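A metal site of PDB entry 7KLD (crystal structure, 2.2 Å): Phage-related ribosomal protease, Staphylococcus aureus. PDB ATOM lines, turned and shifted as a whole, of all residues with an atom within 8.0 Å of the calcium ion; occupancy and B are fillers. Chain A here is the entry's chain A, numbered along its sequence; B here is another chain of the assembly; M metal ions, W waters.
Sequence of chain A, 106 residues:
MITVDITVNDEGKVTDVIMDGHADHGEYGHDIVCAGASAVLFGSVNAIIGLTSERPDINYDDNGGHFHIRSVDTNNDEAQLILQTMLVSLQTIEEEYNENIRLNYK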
ATOM      1  N   MET A   1       3.695 -16.283   3.357  1.00  0.00           N
ATOM      2  CA  MET A   1       2.621 -15.346   3.734  1.00  0.00           C
ATOM      3  C   MET A   1       1.632 -15.186   2.595  1.00  0.00           C
ATOM      4  O   MET A   1       2.033 -14.968   1.450  1.00  0.00           O
ATOM      5  CB  MET A   1       3.192 -13.965   4.110  1.00  0.00           C
ATOM      6  CG  MET A   1       2.143 -12.928   4.528  1.00  0.00           C
ATOM      7  SD  MET A   1       3.024 -11.422   5.115  1.00  0.00           S
ATOM      8  CE  MET A   1       2.711 -11.473   6.864  1.00  0.00           C
ATOM      9  N   ILE A   2       0.332 -15.294   2.888  1.00  0.00           N
ATOM     10  CA  ILE A   2      -0.716 -14.937   1.983  1.00  0.00           C
ATOM     11  C   ILE A   2      -0.957 -13.436   2.178  1.00  0.00           C
ATOM     12  O   ILE A   2      -1.160 -12.990   3.280  1.00  0.00           O
ATOM     13  CB  ILE A   2      -2.064 -15.656   2.274  1.00  0.00           C
ATOM     14  CG1 ILE A   2      -1.920 -17.177   2.367  1.00  0.00           C
ATOM     15  CG2 ILE A   2      -3.139 -15.294   1.246  1.00  0.00           C
ATOM     16  CD1 ILE A   2      -3.160 -17.817   2.951  1.00  0.00           C
ATOM     17  N   ILE A  93      -8.962 -15.401  10.905  1.00  0.00           N
ATOM     18  CA  ILE A  93      -7.820 -16.259  10.898  1.00  0.00           C
ATOM     19  C   ILE A  93      -6.528 -15.503  11.163  1.00  0.00           C
ATOM     20  O   ILE A  93      -5.652 -15.984  11.907  1.00  0.00           O
ATOM     21  CB  ILE A  93      -7.650 -17.020   9.578  1.00  0.00           C
ATOM     22  CG1 ILE A  93      -8.934 -17.761   9.200  1.00  0.00           C
ATOM     23  CG2 ILE A  93      -6.578 -18.087   9.761  1.00  0.00           C
ATOM     24  CD1 ILE A  93      -8.946 -18.210   7.727  1.00  0.00           C
ATOM     25  N   GLU A  94      -6.389 -14.337  10.540  1.00  0.00           N
ATOM     26  CA  GLU A  94      -5.194 -13.502  10.687  1.00  0.00           C
ATOM     27  C   GLU A  94      -4.885 -13.221  12.153  1.00  0.00           C
ATOM     28  O   GLU A  94      -3.734 -13.253  12.583  1.00  0.00           O
ATOM     29  CB  GLU A  94      -5.368 -12.186   9.929  1.00  0.00           C
ATOM     30  CG  GLU A  94      -4.069 -11.434   9.701  1.00  0.00           C
ATOM     31  CD  GLU A  94      -3.585 -10.706  10.946  1.00  0.00           C
ATOM     32  OE1 GLU A  94      -4.434 -10.240  11.731  1.00  0.00           O
ATOM     33  OE2 GLU A  94      -2.353 -10.620  11.135  1.00  0.00           O
ATOM     34  N   GLU A  95      -5.934 -12.940  12.925  1.00  0.00           N
ATOM     35  CA  GLU A  95      -5.792 -12.662  14.337  1.00  0.00           C
ATOM     36  C   GLU A  95      -5.056 -13.779  15.096  1.00  0.00           C
ATOM     37  O   GLU A  95      -4.352 -13.475  15.975  1.00  0.00           O
ATOM     38  CB  GLU A  95      -7.144 -12.336  14.937  1.00  0.00           C
ATOM     39  CG  GLU A  95      -7.133 -11.968  16.400  1.00  0.00           C
ATOM     40  N   TYR A  97      -3.106 -16.207  13.310  1.00  0.00           N
ATOM     41  CA  TYR A  97      -1.980 -16.639  12.492  1.00  0.00           C
ATOM     42  C   TYR A  97      -1.415 -15.397  11.813  1.00  0.00           C
ATOM     43  O   TYR A  97      -1.385 -15.322  10.624  1.00  0.00           O
ATOM     44  CB  TYR A  97      -2.392 -17.725  11.488  1.00  0.00           C
ATOM     45  CG  TYR A  97      -2.915 -18.938  12.157  1.00  0.00           C
ATOM     46  CD1 TYR A  97      -2.057 -19.925  12.576  1.00  0.00           C
ATOM     47  CD2 TYR A  97      -4.244 -19.059  12.479  1.00  0.00           C
ATOM     48  CE1 TYR A  97      -2.517 -21.021  13.236  1.00  0.00           C
ATOM     49  CE2 TYR A  97      -4.706 -20.139  13.157  1.00  0.00           C
ATOM     50  CZ  TYR A  97      -3.838 -21.124  13.527  1.00  0.00           C
ATOM     51  OH  TYR A  97      -4.272 -22.214  14.219  1.00  0.00           O
ATOM     52  N   ASN A  98      -1.024 -14.434  12.638  1.00  0.00           N
ATOM     53  CA  ASN A  98      -0.551 -13.110  12.255  1.00  0.00           C
ATOM     54  C   ASN A  98       0.550 -13.143  11.215  1.00  0.00           C
ATOM     55  O   ASN A  98       0.594 -12.291  10.349  1.00  0.00           O
ATOM     56  CB  ASN A  98       0.069 -12.331  13.444  1.00  0.00           C
ATOM     57  CG  ASN A  98      -0.750 -12.374  14.707  1.00  0.00           C
ATOM     58  OD1 ASN A  98      -0.202 -12.750  15.766  1.00  0.00           O
ATOM     59  ND2 ASN A  98      -2.034 -11.966  14.666  1.00  0.00           N
ATOM     60  N   GLU A  99       1.454 -14.117  11.364  1.00  0.00           N
ATOM     61  CA  GLU A  99       2.614 -14.299  10.529  1.00  0.00           C
ATOM     62  C   GLU A  99       2.335 -14.855   9.129  1.00  0.00           C
ATOM     63  O   GLU A  99       3.195 -14.776   8.248  1.00  0.00           O
ATOM     64  CB  GLU A  99       3.639 -15.207  11.215  1.00  0.00           C
ATOM     65  CG  GLU A  99       4.166 -14.621  12.500  1.00  0.00           C
ATOM     66  CD  GLU A  99       3.420 -15.088  13.760  1.00  0.00           C
ATOM     67  OE1 GLU A  99       2.247 -15.576  13.754  1.00  0.00           O
ATOM     68  OE2 GLU A  99       4.104 -14.972  14.811  1.00  0.00           O
ATOM     69  N   ASN A 100       1.138 -15.438   8.951  1.00  0.00           N
ATOM     70  CA  ASN A 100       0.882 -16.193   7.717  1.00  0.00           C
ATOM     71  C   ASN A 100      -0.122 -15.541   6.801  1.00  0.00           C
ATOM     72  O   ASN A 100      -0.103 -15.830   5.625  1.00  0.00           O
ATOM     73  CB  ASN A 100       0.424 -17.599   8.061  1.00  0.00           C
ATOM     74  CG  ASN A 100       1.289 -18.239   9.137  1.00  0.00           C
ATOM     75  OD1 ASN A 100       0.846 -18.367  10.279  1.00  0.00           O
ATOM     76  ND2 ASN A 100       2.540 -18.598   8.785  1.00  0.00           N
ATOM     77  N   ILE A 101      -0.910 -14.570   7.309  1.00  0.00           N
ATOM     78  CA  ILE A 101      -1.668 -13.652   6.461  1.00  0.00           C
ATOM     79  C   ILE A 101      -1.297 -12.190   6.781  1.00  0.00           C
ATOM     80  O   ILE A 101      -1.078 -11.834   7.927  1.00  0.00           O
ATOM     81  CB  ILE A 101      -3.185 -13.801   6.660  1.00  0.00           C
ATOM     82  CG1 ILE A 101      -3.610 -15.257   6.589  1.00  0.00           C
ATOM     83  CG2 ILE A 101      -3.969 -12.892   5.691  1.00  0.00           C
ATOM     84  CD1 ILE A 101      -5.068 -15.451   6.899  1.00  0.00           C
ATOM     85  N   ARG A 102      -1.337 -11.367   5.729  1.00  0.00           N
ATOM     86  CA  ARG A 102      -1.330  -9.927   5.881  1.00  0.00           C
ATOM     87  C   ARG A 102      -2.594  -9.449   5.197  1.00  0.00           C
ATOM     88  O   ARG A 102      -2.892  -9.867   4.111  1.00  0.00           O
ATOM     89  CB  ARG A 102      -0.118  -9.375   5.184  1.00  0.00           C
ATOM     90  CG  ARG A 102       0.007  -7.845   5.193  1.00  0.00           C
ATOM     91  CD  ARG A 102       1.419  -7.415   4.790  1.00  0.00           C
ATOM     92  NE  ARG A 102       1.557  -7.194   3.340  1.00  0.00           N
ATOM     93  CZ  ARG A 102       1.728  -6.001   2.746  1.00  0.00           C
ATOM     94  NH1 ARG A 102       1.782  -4.880   3.464  1.00  0.00           N
ATOM     95  NH2 ARG A 102       1.838  -5.923   1.432  1.00  0.00           N
ATOM     96  N   LEU A 103      -3.351  -8.602   5.893  1.00  0.00           N
ATOM     97  CA  LEU A 103      -4.426  -7.860   5.284  1.00  0.00           C
ATOM     98  C   LEU A 103      -3.917  -6.429   4.992  1.00  0.00           C
ATOM     99  O   LEU A 103      -3.253  -5.826   5.831  1.00  0.00           O
ATOM    100  CB  LEU A 103      -5.659  -7.812   6.169  1.00  0.00           C
ATOM    101  CG  LEU A 103      -6.471  -9.100   6.380  1.00  0.00           C
ATOM    102  CD1 LEU A 103      -6.867  -9.669   5.042  1.00  0.00           C
ATOM    103  CD2 LEU A 103      -5.764 -10.160   7.200  1.00  0.00           C
ATOM    104  N   ASN B   9      -1.382  -0.287  11.814  1.00  0.00           N
ATOM    105  CA  ASN B   9      -1.307  -0.754  10.442  1.00  0.00           C
ATOM    106  C   ASN B   9      -2.688  -1.306  10.023  1.00  0.00           C
ATOM    107  O   ASN B   9      -3.661  -1.198  10.801  1.00  0.00           O
ATOM    108  CB  ASN B   9      -0.143  -1.747  10.250  1.00  0.00           C
ATOM    109  CG  ASN B   9      -0.391  -3.110  10.898  1.00  0.00           C
ATOM    110  OD1 ASN B   9      -1.473  -3.399  11.412  1.00  0.00           O
ATOM    111  ND2 ASN B   9       0.636  -3.977  10.822  1.00  0.00           N
ATOM    112  N   GLU B  11      -3.814  -4.287   9.755  1.00  0.00           N
ATOM    113  CA  GLU B  11      -4.239  -5.432  10.575  1.00  0.00           C
ATOM    114  C   GLU B  11      -4.545  -5.091  12.025  1.00  0.00           C
ATOM    115  O   GLU B  11      -4.788  -5.970  12.828  1.00  0.00           O
ATOM    116  CB  GLU B  11      -3.158  -6.517  10.549  1.00  0.00           C
ATOM    117  CG  GLU B  11      -2.814  -7.035   9.143  1.00  0.00           C
ATOM    118  CD  GLU B  11      -1.909  -8.241   9.209  1.00  0.00           C
ATOM    119  OE1 GLU B  11      -1.014  -8.267  10.041  1.00  0.00           O
ATOM    120  OE2 GLU B  11      -2.100  -9.215   8.482  1.00  0.00           O
ATOM    121  N   LYS B  13      -2.420  -3.855  14.179  1.00  0.00           N
ATOM    122  CA  LYS B  13      -1.252  -3.786  15.063  1.00  0.00           C
ATOM    123  C   LYS B  13      -0.760  -2.309  15.158  1.00  0.00           C
ATOM    124  O   LYS B  13      -0.697  -1.574  14.145  1.00  0.00           O
ATOM    125  CB  LYS B  13      -0.069  -4.638  14.572  1.00  0.00           C
ATOM    126  CG  LYS B  13      -0.439  -5.958  13.903  1.00  0.00           C
ATOM    127  CD  LYS B  13      -0.600  -7.099  14.906  1.00  0.00           C
ATOM    128  CE  LYS B  13      -0.939  -8.396  14.185  1.00  0.00           C
ATOM    129  NZ  LYS B  13      -2.304  -8.278  13.576  1.00  0.00           N
ATOM    130  N   THR B  74       5.999  -6.821  15.280  1.00  0.00           N
ATOM    131  CA  THR B  74       4.551  -6.616  15.240  1.00  0.00           C
ATOM    132  C   THR B  74       3.792  -7.925  15.427  1.00  0.00           C
ATOM    133  O   THR B  74       2.585  -7.895  15.579  1.00  0.00           O
ATOM    134  CB  THR B  74       4.065  -5.960  13.931  1.00  0.00           C
ATOM    135  OG1 THR B  74       4.676  -6.606  12.794  1.00  0.00           O
ATOM    136  CG2 THR B  74       4.343  -4.434  13.891  1.00  0.00           C
ATOM    137  N   ASN B  75       4.478  -9.057  15.224  1.00  0.00           N
ATOM    138  CA  ASN B  75       3.876 -10.371  15.403  1.00  0.00           C
ATOM    139  C   ASN B  75       4.056 -10.939  16.830  1.00  0.00           C
ATOM    140  O   ASN B  75       3.687 -12.082  17.068  1.00  0.00           O
ATOM    141  CB  ASN B  75       4.347 -11.395  14.402  1.00  0.00           C
ATOM    142  CG  ASN B  75       3.866 -11.095  12.984  1.00  0.00           C
ATOM    143  OD1 ASN B  75       2.699 -10.797  12.804  1.00  0.00           O
ATOM    144  ND2 ASN B  75       4.742 -11.209  11.976  1.00  0.00           N
HETATM  145 CA    CA M   1      -0.408 -10.464   9.818  1.00  0.00          CA
HETATM  146  O   HOH W   1       1.168  -9.422  11.486  1.00  0.00           O
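Within 4 Å of the calcium ion: Glu 94, Asn 98, Ile 101 and Glu 11 of chain B. Along chain A the residues within 4 Å of the calcium ion span positions 94 to 101. The nearest printed residue that does not touch the calcium ion is Arg 102 (4.1 Å).
O of Asn 98 binds the calcium ion (2.2 Å). The side-chain carboxylate (OE1) of Glu 11 of chain B is bound to the calcium ion, 2.3 Å away. OE2 of Glu 94 is bound to the calcium ion (2.4 Å). The backbone carbonyl oxygen (O) of Ile 101 is bound to the calcium ion (2.4 Å). The calcium ion is bound by OE2 of Glu 11 of chain B (2.5 Å). The calcium ion is bound by water W1, at 2.5 Å. The calcium ion has six donor atoms within binding distance.
The backbone carbonyl oxygen (O) of Glu 11 of chain B sits at hydrogen-bond distance from the side-chain amino group (NZ) of Lys 13 of chain B, 3.5 Å away. The side-chain carboxylate of Glu 11 of chain B sits close to the backbone NH of Leu 103, at 2.9 Å. ND2 of Asn 98 lies within hydrogen-bond range of O of Glu 95, 3.1 Å away. The backbone NH of Glu 11 of chain B lies within hydrogen-bond range of the side-chain amide oxygen of Asn 9 of chain B. The side-chain carboxylate (OE1) of Glu 94 lies within salt-bridge range of the side-chain amino group (NZ) of Lys 13 of chain B (3.4 Å).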
